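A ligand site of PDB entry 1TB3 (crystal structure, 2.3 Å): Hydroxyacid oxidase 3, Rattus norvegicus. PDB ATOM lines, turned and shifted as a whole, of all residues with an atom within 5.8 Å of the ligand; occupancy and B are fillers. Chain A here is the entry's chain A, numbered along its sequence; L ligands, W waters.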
ATOM      1  N   PHE A  23       8.222 -16.349   7.899  1.00  0.00           N
ATOM      2  CA  PHE A  23       8.696 -15.461   6.842  1.00  0.00           C
ATOM      3  C   PHE A  23       7.836 -14.197   6.735  1.00  0.00           C
ATOM      4  O   PHE A  23       8.348 -13.113   6.443  1.00  0.00           O
ATOM      5  CB  PHE A  23       8.681 -16.191   5.498  1.00  0.00           C
ATOM      6  CG  PHE A  23       8.864 -15.276   4.317  1.00  0.00           C
ATOM      7  CD1 PHE A  23       7.776 -14.936   3.516  1.00  0.00           C
ATOM      8  CD2 PHE A  23      10.104 -14.709   4.037  1.00  0.00           C
ATOM      9  CE1 PHE A  23       7.927 -14.060   2.446  1.00  0.00           C
ATOM     10  CE2 PHE A  23      10.269 -13.827   2.967  1.00  0.00           C
ATOM     11  CZ  PHE A  23       9.174 -13.506   2.166  1.00  0.00           C
ATOM     12  N   ILE A  24       6.537 -14.340   6.976  1.00  0.00           N
ATOM     13  CA  ILE A  24       5.625 -13.216   6.912  1.00  0.00           C
ATOM     14  C   ILE A  24       5.791 -12.321   8.135  1.00  0.00           C
ATOM     15  O   ILE A  24       5.546 -11.118   8.056  1.00  0.00           O
ATOM     16  CB  ILE A  24       4.170 -13.707   6.759  1.00  0.00           C
ATOM     17  CG1 ILE A  24       3.993 -14.305   5.353  1.00  0.00           C
ATOM     18  CG2 ILE A  24       3.195 -12.563   6.983  1.00  0.00           C
ATOM     19  CD1 ILE A  24       2.697 -15.044   5.158  1.00  0.00           C
ATOM     20  N   GLU A  25       6.214 -12.892   9.248  1.00  0.00           N
ATOM     21  CA  GLU A  25       6.463 -12.122  10.470  1.00  0.00           C
ATOM     22  C   GLU A  25       7.832 -11.483  10.252  1.00  0.00           C
ATOM     23  O   GLU A  25       7.987 -10.252  10.249  1.00  0.00           O
ATOM     24  CB  GLU A  25       6.504 -13.064  11.671  1.00  0.00           C
ATOM     25  CG  GLU A  25       5.119 -13.533  12.112  1.00  0.00           C
ATOM     26  CD  GLU A  25       4.366 -12.456  12.878  1.00  0.00           C
ATOM     27  OE1 GLU A  25       4.620 -12.326  14.096  1.00  0.00           O
ATOM     28  OE2 GLU A  25       3.560 -11.713  12.273  1.00  0.00           O
ATOM     29  N   ASN A  37       6.300  -0.671  16.314  1.00  0.00           N
ATOM     30  CA  ASN A  37       5.426  -0.062  15.321  1.00  0.00           C
ATOM     31  C   ASN A  37       3.986  -0.052  15.830  1.00  0.00           C
ATOM     32  O   ASN A  37       3.212   0.857  15.520  1.00  0.00           O
ATOM     33  CB  ASN A  37       5.496  -0.790  13.981  1.00  0.00           C
ATOM     34  CG  ASN A  37       6.672  -0.321  13.100  1.00  0.00           C
ATOM     35  OD1 ASN A  37       7.205   0.778  13.279  1.00  0.00           O
ATOM     36  ND2 ASN A  37       7.047  -1.150  12.138  1.00  0.00           N
ATOM     37  N   SER A  75       0.777  -2.018   0.577  1.00  0.00           N
ATOM     38  CA  SER A  75       2.202  -1.833   0.430  1.00  0.00           C
ATOM     39  C   SER A  75       2.790  -3.041  -0.298  1.00  0.00           C
ATOM     40  O   SER A  75       2.211  -4.119  -0.290  1.00  0.00           O
ATOM     41  CB  SER A  75       2.858  -1.684   1.804  1.00  0.00           C
ATOM     42  OG  SER A  75       3.589  -0.468   1.866  1.00  0.00           O
ATOM     43  N   PRO A  76       3.937  -2.853  -0.958  1.00  0.00           N
ATOM     44  CA  PRO A  76       4.541  -3.982  -1.679  1.00  0.00           C
ATOM     45  C   PRO A  76       4.973  -5.124  -0.753  1.00  0.00           C
ATOM     46  O   PRO A  76       5.669  -4.893   0.249  1.00  0.00           O
ATOM     47  CB  PRO A  76       5.721  -3.329  -2.406  1.00  0.00           C
ATOM     48  CG  PRO A  76       6.093  -2.175  -1.485  1.00  0.00           C
ATOM     49  CD  PRO A  76       4.743  -1.637  -1.103  1.00  0.00           C
ATOM     50  N   THR A  77       4.544  -6.338  -1.063  1.00  0.00           N
ATOM     51  CA  THR A  77       4.902  -7.533  -0.299  1.00  0.00           C
ATOM     52  C   THR A  77       5.113  -8.675  -1.286  1.00  0.00           C
ATOM     53  O   THR A  77       4.233  -8.973  -2.093  1.00  0.00           O
ATOM     54  CB  THR A  77       3.814  -7.945   0.713  1.00  0.00           C
ATOM     55  OG1 THR A  77       2.525  -7.933   0.077  1.00  0.00           O
ATOM     56  CG2 THR A  77       3.836  -7.009   1.919  1.00  0.00           C
ATOM     57  N   ALA A  78       6.300  -9.271  -1.221  1.00  0.00           N
ATOM     58  CA  ALA A  78       6.670 -10.341  -2.134  1.00  0.00           C
ATOM     59  C   ALA A  78       5.943 -11.658  -1.952  1.00  0.00           C
ATOM     60  O   ALA A  78       5.391 -11.933  -0.893  1.00  0.00           O
ATOM     61  CB  ALA A  78       8.177 -10.604  -2.040  1.00  0.00           C
ATOM     62  N   ILE A  82       2.493 -17.704  -1.286  1.00  0.00           N
ATOM     63  CA  ILE A  82       2.769 -18.496  -0.100  1.00  0.00           C
ATOM     64  C   ILE A  82       1.560 -18.400   0.816  1.00  0.00           C
ATOM     65  O   ILE A  82       1.466 -19.128   1.803  1.00  0.00           O
ATOM     66  CB  ILE A  82       4.002 -18.017   0.685  1.00  0.00           C
ATOM     67  CG1 ILE A  82       3.773 -16.614   1.219  1.00  0.00           C
ATOM     68  CG2 ILE A  82       5.243 -18.082  -0.202  1.00  0.00           C
ATOM     69  CD1 ILE A  82       4.916 -16.111   2.059  1.00  0.00           C
ATOM     70  N   SER A 105       4.872  -5.825  -5.638  1.00  0.00           N
ATOM     71  CA  SER A 105       6.259  -6.114  -5.286  1.00  0.00           C
ATOM     72  C   SER A 105       7.116  -6.495  -6.487  1.00  0.00           C
ATOM     73  O   SER A 105       6.641  -7.029  -7.477  1.00  0.00           O
ATOM     74  CB  SER A 105       6.306  -7.243  -4.248  1.00  0.00           C
ATOM     75  OG  SER A 105       7.645  -7.656  -4.034  1.00  0.00           O
ATOM     76  N   SER A 106       8.405  -6.233  -6.362  1.00  0.00           N
ATOM     77  CA  SER A 106       9.367  -6.563  -7.400  1.00  0.00           C
ATOM     78  C   SER A 106       9.569  -8.082  -7.431  1.00  0.00           C
ATOM     79  O   SER A 106      10.117  -8.632  -8.377  1.00  0.00           O
ATOM     80  CB  SER A 106      10.700  -5.855  -7.101  1.00  0.00           C
ATOM     81  OG  SER A 106      11.650  -6.094  -8.113  1.00  0.00           O
ATOM     82  N   TYR A 107       9.115  -8.764  -6.371  1.00  0.00           N
ATOM     83  CA  TYR A 107       9.263 -10.207  -6.277  1.00  0.00           C
ATOM     84  C   TYR A 107       7.928 -10.914  -6.155  1.00  0.00           C
ATOM     85  O   TYR A 107       7.711 -11.696  -5.221  1.00  0.00           O
ATOM     86  CB  TYR A 107      10.127 -10.573  -5.073  1.00  0.00           C
ATOM     87  CG  TYR A 107      11.519  -9.992  -5.128  1.00  0.00           C
ATOM     88  CD1 TYR A 107      12.344 -10.209  -6.226  1.00  0.00           C
ATOM     89  CD2 TYR A 107      12.010  -9.228  -4.075  1.00  0.00           C
ATOM     90  CE1 TYR A 107      13.637  -9.698  -6.281  1.00  0.00           C
ATOM     91  CE2 TYR A 107      13.305  -8.706  -4.111  1.00  0.00           C
ATOM     92  CZ  TYR A 107      14.102  -8.946  -5.220  1.00  0.00           C
ATOM     93  OH  TYR A 107      15.390  -8.443  -5.255  1.00  0.00           O
ATOM     94  N   GLN A 127       6.773  -1.450  -7.365  1.00  0.00           N
ATOM     95  CA  GLN A 127       7.968  -1.338  -6.537  1.00  0.00           C
ATOM     96  C   GLN A 127       9.058  -2.121  -7.261  1.00  0.00           C
ATOM     97  O   GLN A 127       8.989  -3.343  -7.395  1.00  0.00           O
ATOM     98  CB  GLN A 127       7.711  -1.924  -5.142  1.00  0.00           C
ATOM     99  CG  GLN A 127       8.857  -1.801  -4.147  1.00  0.00           C
ATOM    100  CD  GLN A 127       9.757  -3.028  -4.130  1.00  0.00           C
ATOM    101  OE1 GLN A 127       9.273  -4.160  -4.065  1.00  0.00           O
ATOM    102  NE2 GLN A 127      11.062  -2.808  -4.173  1.00  0.00           N
ATOM    103  N   TYR A 129      13.121  -3.058  -7.531  1.00  0.00           N
ATOM    104  CA  TYR A 129      14.444  -3.073  -6.943  1.00  0.00           C
ATOM    105  C   TYR A 129      15.428  -2.882  -8.091  1.00  0.00           C
ATOM    106  O   TYR A 129      15.579  -3.755  -8.951  1.00  0.00           O
ATOM    107  CB  TYR A 129      14.715  -4.397  -6.208  1.00  0.00           C
ATOM    108  CG  TYR A 129      14.170  -4.474  -4.795  1.00  0.00           C
ATOM    109  CD1 TYR A 129      13.121  -5.332  -4.475  1.00  0.00           C
ATOM    110  CD2 TYR A 129      14.713  -3.687  -3.772  1.00  0.00           C
ATOM    111  CE1 TYR A 129      12.632  -5.421  -3.170  1.00  0.00           C
ATOM    112  CE2 TYR A 129      14.227  -3.767  -2.457  1.00  0.00           C
ATOM    113  CZ  TYR A 129      13.194  -4.642  -2.166  1.00  0.00           C
ATOM    114  OH  TYR A 129      12.724  -4.738  -0.869  1.00  0.00           O
ATOM    115  N   THR A 155      12.323   1.326  -3.093  1.00  0.00           N
ATOM    116  CA  THR A 155      12.553   1.001  -1.698  1.00  0.00           C
ATOM    117  C   THR A 155      14.037   1.207  -1.433  1.00  0.00           C
ATOM    118  O   THR A 155      14.881   0.558  -2.042  1.00  0.00           O
ATOM    119  CB  THR A 155      12.099  -0.455  -1.408  1.00  0.00           C
ATOM    120  OG1 THR A 155      10.673  -0.541  -1.556  1.00  0.00           O
ATOM    121  CG2 THR A 155      12.478  -0.864   0.016  1.00  0.00           C
ATOM    122  N   ASP A 157      15.541   1.151   1.879  1.00  0.00           N
ATOM    123  CA  ASP A 157      16.076   0.586   3.117  1.00  0.00           C
ATOM    124  C   ASP A 157      16.495  -0.875   3.013  1.00  0.00           C
ATOM    125  O   ASP A 157      16.613  -1.573   4.017  1.00  0.00           O
ATOM    126  CB  ASP A 157      15.037   0.743   4.248  1.00  0.00           C
ATOM    127  CG  ASP A 157      13.708   0.045   3.939  1.00  0.00           C
ATOM    128  OD1 ASP A 157      12.716   0.355   4.636  1.00  0.00           O
ATOM    129  OD2 ASP A 157      13.643  -0.816   3.029  1.00  0.00           O
ATOM    130  N   THR A 158      16.740  -1.334   1.799  1.00  0.00           N
ATOM    131  CA  THR A 158      17.113  -2.727   1.611  1.00  0.00           C
ATOM    132  C   THR A 158      18.323  -2.941   0.689  1.00  0.00           C
ATOM    133  O   THR A 158      18.259  -3.686  -0.275  1.00  0.00           O
ATOM    134  CB  THR A 158      15.899  -3.526   1.070  1.00  0.00           C
ATOM    135  OG1 THR A 158      14.747  -3.230   1.871  1.00  0.00           O
ATOM    136  CG2 THR A 158      16.158  -5.021   1.141  1.00  0.00           C
ATOM    137  N   LYS A 223      10.484   4.853  -0.718  1.00  0.00           N
ATOM    138  CA  LYS A 223       9.962   4.113   0.431  1.00  0.00           C
ATOM    139  C   LYS A 223      11.046   3.704   1.425  1.00  0.00           C
ATOM    140  O   LYS A 223      12.029   3.065   1.062  1.00  0.00           O
ATOM    141  CB  LYS A 223       9.211   2.861  -0.052  1.00  0.00           C
ATOM    142  CG  LYS A 223       8.622   1.952   1.022  1.00  0.00           C
ATOM    143  CD  LYS A 223       7.758   0.864   0.367  1.00  0.00           C
ATOM    144  CE  LYS A 223       7.271  -0.190   1.351  1.00  0.00           C
ATOM    145  NZ  LYS A 223       8.338  -1.115   1.824  1.00  0.00           N
ATOM    146  N   SER A 245       8.661   4.600   6.346  1.00  0.00           N
ATOM    147  CA  SER A 245       8.574   3.193   6.680  1.00  0.00           C
ATOM    148  C   SER A 245       9.889   2.637   7.189  1.00  0.00           C
ATOM    149  O   SER A 245      10.956   3.159   6.852  1.00  0.00           O
ATOM    150  CB  SER A 245       8.150   2.433   5.420  1.00  0.00           C
ATOM    151  OG  SER A 245       8.435   1.046   5.508  1.00  0.00           O
ATOM    152  N   ASN A 246       9.808   1.592   8.008  1.00  0.00           N
ATOM    153  CA  ASN A 246      10.993   0.912   8.507  1.00  0.00           C
ATOM    154  C   ASN A 246      10.924  -0.542   8.031  1.00  0.00           C
ATOM    155  O   ASN A 246      11.468  -1.445   8.672  1.00  0.00           O
ATOM    156  CB  ASN A 246      11.099   0.975  10.031  1.00  0.00           C
ATOM    157  CG  ASN A 246       9.803   0.587  10.733  1.00  0.00           C
ATOM    158  OD1 ASN A 246       9.116  -0.355  10.331  1.00  0.00           O
ATOM    159  ND2 ASN A 246       9.481   1.314  11.802  1.00  0.00           N
ATOM    160  N   HIS A 247      10.211  -0.749   6.927  1.00  0.00           N
ATOM    161  CA  HIS A 247      10.074  -2.086   6.334  1.00  0.00           C
ATOM    162  C   HIS A 247       9.498  -3.087   7.341  1.00  0.00           C
ATOM    163  O   HIS A 247       9.907  -4.253   7.386  1.00  0.00           O
ATOM    164  CB  HIS A 247      11.452  -2.562   5.851  1.00  0.00           C
ATOM    165  CG  HIS A 247      11.409  -3.437   4.642  1.00  0.00           C
ATOM    166  ND1 HIS A 247      11.734  -2.969   3.385  1.00  0.00           N
ATOM    167  CD2 HIS A 247      11.108  -4.747   4.491  1.00  0.00           C
ATOM    168  CE1 HIS A 247      11.651  -3.960   2.510  1.00  0.00           C
ATOM    169  NE2 HIS A 247      11.276  -5.053   3.158  1.00  0.00           N
ATOM    170  N   GLY A 248       8.567  -2.614   8.174  1.00  0.00           N
ATOM    171  CA  GLY A 248       7.947  -3.472   9.164  1.00  0.00           C
ATOM    172  C   GLY A 248       8.890  -4.127  10.152  1.00  0.00           C
ATOM    173  O   GLY A 248       8.603  -5.201  10.684  1.00  0.00           O
ATOM    174  N   ARG A 250      11.656  -5.479   9.503  1.00  0.00           N
ATOM    175  CA  ARG A 250      12.297  -6.639   8.875  1.00  0.00           C
ATOM    176  C   ARG A 250      13.706  -6.320   8.361  1.00  0.00           C
ATOM    177  O   ARG A 250      14.399  -7.198   7.865  1.00  0.00           O
ATOM    178  CB  ARG A 250      11.444  -7.127   7.696  1.00  0.00           C
ATOM    179  CG  ARG A 250      10.006  -7.514   8.092  1.00  0.00           C
ATOM    180  CD  ARG A 250       9.093  -7.523   6.881  1.00  0.00           C
ATOM    181  NE  ARG A 250       9.466  -8.512   5.875  1.00  0.00           N
ATOM    182  CZ  ARG A 250       9.158  -9.803   5.954  1.00  0.00           C
ATOM    183  NH1 ARG A 250       8.464 -10.271   6.985  1.00  0.00           N
ATOM    184  NH2 ARG A 250       9.534 -10.631   4.981  1.00  0.00           N
ATOM    185  N   ASP A 278       3.623   3.322   6.444  1.00  0.00           N
ATOM    186  CA  ASP A 278       3.184   1.955   6.670  1.00  0.00           C
ATOM    187  C   ASP A 278       3.930   1.472   7.903  1.00  0.00           C
ATOM    188  O   ASP A 278       4.846   2.143   8.366  1.00  0.00           O
ATOM    189  CB  ASP A 278       3.425   1.041   5.455  1.00  0.00           C
ATOM    190  CG  ASP A 278       4.880   0.619   5.273  1.00  0.00           C
ATOM    191  OD1 ASP A 278       5.140  -0.011   4.218  1.00  0.00           O
ATOM    192  OD2 ASP A 278       5.760   0.865   6.132  1.00  0.00           O
ATOM    193  N   GLY A 279       3.514   0.338   8.442  1.00  0.00           N
ATOM    194  CA  GLY A 279       4.176  -0.179   9.633  1.00  0.00           C
ATOM    195  C   GLY A 279       3.284  -0.156  10.866  1.00  0.00           C
ATOM    196  O   GLY A 279       3.158   0.873  11.531  1.00  0.00           O
ATOM    197  N   GLY A 280       2.657  -1.295  11.146  1.00  0.00           N
ATOM    198  CA  GLY A 280       1.806  -1.406  12.326  1.00  0.00           C
ATOM    199  C   GLY A 280       0.379  -0.916  12.256  1.00  0.00           C
ATOM    200  O   GLY A 280      -0.291  -0.872  13.287  1.00  0.00           O
ATOM    201  N   VAL A 281      -0.105  -0.526  11.067  1.00  0.00           N
ATOM    202  CA  VAL A 281      -1.483  -0.054  10.960  1.00  0.00           C
ATOM    203  C   VAL A 281      -2.354  -1.311  11.063  1.00  0.00           C
ATOM    204  O   VAL A 281      -2.210  -2.223  10.265  1.00  0.00           O
ATOM    205  CB  VAL A 281      -1.753   0.636   9.588  1.00  0.00           C
ATOM    206  CG1 VAL A 281      -3.218   1.076   9.498  1.00  0.00           C
ATOM    207  CG2 VAL A 281      -0.832   1.842   9.419  1.00  0.00           C
ATOM    208  N   ARG A 282      -3.240  -1.340  12.058  1.00  0.00           N
ATOM    209  CA  ARG A 282      -4.099  -2.513  12.279  1.00  0.00           C
ATOM    210  C   ARG A 282      -5.543  -2.156  12.604  1.00  0.00           C
ATOM    211  O   ARG A 282      -6.438  -2.966  12.398  1.00  0.00           O
ATOM    212  CB  ARG A 282      -3.547  -3.375  13.419  1.00  0.00           C
ATOM    213  CG  ARG A 282      -2.096  -3.806  13.248  1.00  0.00           C
ATOM    214  CD  ARG A 282      -1.932  -4.776  12.102  1.00  0.00           C
ATOM    215  NE  ARG A 282      -0.553  -5.254  11.969  1.00  0.00           N
ATOM    216  CZ  ARG A 282       0.328  -4.774  11.096  1.00  0.00           C
ATOM    217  NH1 ARG A 282      -0.025  -3.818  10.241  1.00  0.00           N
ATOM    218  NH2 ARG A 282       1.556  -5.270  11.068  1.00  0.00           N
ATOM    219  N   PHE A 299      -0.303   2.529   4.065  1.00  0.00           N
ATOM    220  CA  PHE A 299      -0.221   1.300   3.296  1.00  0.00           C
ATOM    221  C   PHE A 299      -0.153   0.131   4.277  1.00  0.00           C
ATOM    222  O   PHE A 299       0.407   0.265   5.378  1.00  0.00           O
ATOM    223  CB  PHE A 299       1.016   1.279   2.378  1.00  0.00           C
ATOM    224  CG  PHE A 299       0.922   2.230   1.224  1.00  0.00           C
ATOM    225  CD1 PHE A 299       1.074   3.604   1.416  1.00  0.00           C
ATOM    226  CD2 PHE A 299       0.689   1.761  -0.059  1.00  0.00           C
ATOM    227  CE1 PHE A 299       0.976   4.496   0.354  1.00  0.00           C
ATOM    228  CE2 PHE A 299       0.588   2.642  -1.141  1.00  0.00           C
ATOM    229  CZ  PHE A 299       0.726   4.012  -0.930  1.00  0.00           C
ATOM    230  N   LEU A 300      -0.737  -0.998   3.877  1.00  0.00           N
ATOM    231  CA  LEU A 300      -0.778  -2.196   4.705  1.00  0.00           C
ATOM    232  C   LEU A 300       0.160  -3.260   4.136  1.00  0.00           C
ATOM    233  O   LEU A 300       0.146  -3.550   2.945  1.00  0.00           O
ATOM    234  CB  LEU A 300      -2.195  -2.759   4.747  1.00  0.00           C
ATOM    235  CG  LEU A 300      -3.287  -1.883   5.337  1.00  0.00           C
ATOM    236  CD1 LEU A 300      -4.657  -2.513   5.073  1.00  0.00           C
ATOM    237  CD2 LEU A 300      -3.037  -1.692   6.822  1.00  0.00           C
ATOM    238  N   GLY A 301       0.951  -3.852   5.025  1.00  0.00           N
ATOM    239  CA  GLY A 301       1.854  -4.900   4.605  1.00  0.00           C
ATOM    240  C   GLY A 301       1.271  -6.266   4.935  1.00  0.00           C
ATOM    241  O   GLY A 301       0.504  -6.838   4.154  1.00  0.00           O
ATOM    242  N   ARG A 302       1.614  -6.785   6.113  1.00  0.00           N
ATOM    243  CA  ARG A 302       1.158  -8.110   6.527  1.00  0.00           C
ATOM    244  C   ARG A 302      -0.351  -8.375   6.503  1.00  0.00           C
ATOM    245  O   ARG A 302      -0.770  -9.436   6.067  1.00  0.00           O
ATOM    246  CB  ARG A 302       1.707  -8.432   7.926  1.00  0.00           C
ATOM    247  CG  ARG A 302       3.236  -8.427   8.020  1.00  0.00           C
ATOM    248  CD  ARG A 302       3.687  -8.725   9.424  1.00  0.00           C
ATOM    249  NE  ARG A 302       5.135  -8.636   9.602  1.00  0.00           N
ATOM    250  CZ  ARG A 302       5.818  -7.506   9.766  1.00  0.00           C
ATOM    251  NH1 ARG A 302       5.198  -6.326   9.773  1.00  0.00           N
ATOM    252  NH2 ARG A 302       7.127  -7.558   9.984  1.00  0.00           N
ATOM    253  N   PRO A 303      -1.176  -7.430   6.951  1.00  0.00           N
ATOM    254  CA  PRO A 303      -2.624  -7.674   6.940  1.00  0.00           C
ATOM    255  C   PRO A 303      -3.157  -8.185   5.605  1.00  0.00           C
ATOM    256  O   PRO A 303      -4.071  -9.015   5.590  1.00  0.00           O
ATOM    257  CB  PRO A 303      -3.207  -6.327   7.342  1.00  0.00           C
ATOM    258  CG  PRO A 303      -2.149  -5.781   8.266  1.00  0.00           C
ATOM    259  CD  PRO A 303      -0.870  -6.101   7.522  1.00  0.00           C
ATOM    260  N   LEU A 305      -1.567 -10.054   3.464  1.00  0.00           N
ATOM    261  CA  LEU A 305      -1.214 -11.459   3.365  1.00  0.00           C
ATOM    262  C   LEU A 305      -2.109 -12.294   4.302  1.00  0.00           C
ATOM    263  O   LEU A 305      -2.514 -13.391   3.938  1.00  0.00           O
ATOM    264  CB  LEU A 305       0.267 -11.665   3.717  1.00  0.00           C
ATOM    265  CG  LEU A 305       1.269 -10.942   2.819  1.00  0.00           C
ATOM    266  CD1 LEU A 305       2.675 -11.148   3.348  1.00  0.00           C
ATOM    267  CD2 LEU A 305       1.155 -11.458   1.382  1.00  0.00           C
HETATM  268  N1  LIG L   1       8.689  -4.218   0.971  1.00  0.00           N
HETATM  269  C1  LIG L   1       9.216  -3.832  -0.244  1.00  0.00           C
HETATM  270  O1  LIG L   1       9.542  -2.670  -0.527  1.00  0.00           O
HETATM  271  N2  LIG L   1       9.338  -4.908  -1.137  1.00  0.00           N
HETATM  272  C2  LIG L   1       8.994  -6.246  -0.898  1.00  0.00           C
HETATM  273  O2  LIG L   1       9.191  -7.031  -1.829  1.00  0.00           O
HETATM  274  C3  LIG L   1       8.446  -6.493   0.441  1.00  0.00           C
HETATM  275  N3  LIG L   1       8.067  -7.827   0.749  1.00  0.00           N
HETATM  276  C4  LIG L   1       7.509  -8.116   1.999  1.00  0.00           C
HETATM  277  C5  LIG L   1       7.124  -9.417   2.255  1.00  0.00           C
HETATM  278  C6  LIG L   1       6.541  -9.751   3.476  1.00  0.00           C
HETATM  279  C7  LIG L   1       6.129 -11.192   3.697  1.00  0.00           C
HETATM  280  C8  LIG L   1       6.347  -8.743   4.459  1.00  0.00           C
HETATM  281  C9  LIG L   1       5.729  -9.041   5.767  1.00  0.00           C
HETATM  282  C10 LIG L   1       6.741  -7.444   4.223  1.00  0.00           C
HETATM  283  C11 LIG L   1       7.328  -7.102   2.983  1.00  0.00           C
HETATM  284  N4  LIG L   1       7.732  -5.756   2.675  1.00  0.00           N
HETATM  285  C12 LIG L   1       8.287  -5.477   1.406  1.00  0.00           C
HETATM  286  C13 LIG L   1       7.583  -4.723   3.569  1.00  0.00           C
HETATM  287  C14 LIG L   1       6.258  -3.912   3.360  1.00  0.00           C
HETATM  288  O3  LIG L   1       6.381  -3.199   2.135  1.00  0.00           O
HETATM  289  C15 LIG L   1       5.975  -2.920   4.490  1.00  0.00           C
HETATM  290  O4  LIG L   1       7.079  -2.018   4.601  1.00  0.00           O
HETATM  291  C16 LIG L   1       5.769  -3.514   5.868  1.00  0.00           C
HETATM  292  O5  LIG L   1       5.477  -4.917   5.901  1.00  0.00           O
HETATM  293  C17 LIG L   1       4.607  -2.752   6.409  1.00  0.00           C
HETATM  294  O6  LIG L   1       4.239  -3.098   7.699  1.00  0.00           O
HETATM  295  P1  LIG L   1       3.045  -3.889   8.191  1.00  0.00           P
HETATM  296  O7  LIG L   1       3.065  -3.574   9.632  1.00  0.00           O
HETATM  297  O8  LIG L   1       3.297  -5.266   7.796  1.00  0.00           O
HETATM  298  O9  LIG L   1       1.869  -3.355   7.528  1.00  0.00           O
HETATM  299  O   HOH W   1       5.445  -3.645  11.288  1.00  0.00           O
HETATM  300  O   HOH W   2       1.152  -0.922   7.801  1.00  0.00           O
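Water W2 lies within hydrogen-bond range of O9 of the ligand, N of Gly 279 and O of Phe 299.
Water W1 lies within hydrogen-bond range of an oxygen (O7) of the ligand, the side-chain amide nitrogen of Asn 37 and the guanidinium group of Arg 302.
O1 of the ligand lies within hydrogen-bond range of OG1 of Thr 155, 2.6 Å away.
O of Pro 76 sits at hydrogen-bond distance from O3 of the ligand, 2.6 Å away.
An oxygen (O7) of the ligand is in salt-bridge range of the guanidinium group of Arg 282 (2.7 Å).
An oxygen (O9) of the ligand is in hydrogen-bond range of the backbone NH of Gly 301 (2.7 Å).
The side-chain hydroxyl (OG) of Ser 105 lies within hydrogen-bond range of an oxygen (O2) of the ligand (2.8 Å).
N of Gly 280 sits at hydrogen-bond distance from O7 of the ligand (2.8 Å).
OD1 of Asp 278 sits at hydrogen-bond distance from O4 of the ligand (2.8 Å).
N of Arg 302 sits at hydrogen-bond distance from O8 of the ligand (2.8 Å).
An oxygen (O8) of the ligand lies within salt-bridge range of the guanidinium group of Arg 302, at 2.9 Å.
The side-chain amino group (NZ) of Lys 223 sits at hydrogen-bond distance from an oxygen (O3) of the ligand, at 2.9 Å.
N of Ala 78 sits at hydrogen-bond distance from N3 of the ligand (3.0 Å).
The side-chain amide oxygen of Gln 127 lies within hydrogen-bond range of a nitrogen (N2) of the ligand, at 3.0 Å.
A ring nitrogen (NE2) of His 247 sits close to a nitrogen (N1) of the ligand (3.5 Å).
The side-chain hydroxyl of Tyr 129 lies within hydrogen-bond range of a nitrogen (N2) of the ligand, 3.4 Å away.
O4 of the ligand lies within hydrogen-bond range of OG of Ser 245 (3.5 Å).
The side-chain carboxylate (OD2) of Asp 278 sits at hydrogen-bond distance from the side-chain hydroxyl (OG) of Ser 245 (2.8 Å).
O of Gly 248 sits at hydrogen-bond distance from NH2 of Arg 302 (2.9 Å).
The guanidinium group of Arg 302 lies within hydrogen-bond range of the backbone carbonyl oxygen of Glu 25 (2.8 Å).
O of Ile 24 sits at hydrogen-bond distance from NH1 of Arg 250 (3.2 Å).
OG of Ser 245 sits at hydrogen-bond distance from N of His 247, 2.9 Å away.
A ring nitrogen (ND1) of His 247 lies close to the side-chain hydroxyl of Thr 158 (3.4 Å).
OD1 of Asn 246 sits close to N of Gly 248, 3.2 Å away.
O of Leu 300 lies within hydrogen-bond range of N of Ser 75 (2.9 Å).
Residues that only touch the ligand: Phe 23 (3.6 Å), Ile 24 (3.1 Å), Ser 75 (3.8 Å), Thr 77 (3.3 Å), Gly 248 (3.7 Å), Arg 250 (3.2 Å), Gly 279 (3.5 Å), Leu 300 (3.8 Å), Pro 303 (3.9 Å) and Leu 305 (3.5 Å).
Hydrophobic or aromatic side chains that line the ligand: Phe 23, Pro 76, Ala 78, Tyr 129, His 247, Pro 303 and Leu 305.
Of the 34 residues printed, 24 come within 4 Å of the ligand.
The nearest printed residue that does not touch the ligand is Tyr 107 (4.2 Å).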
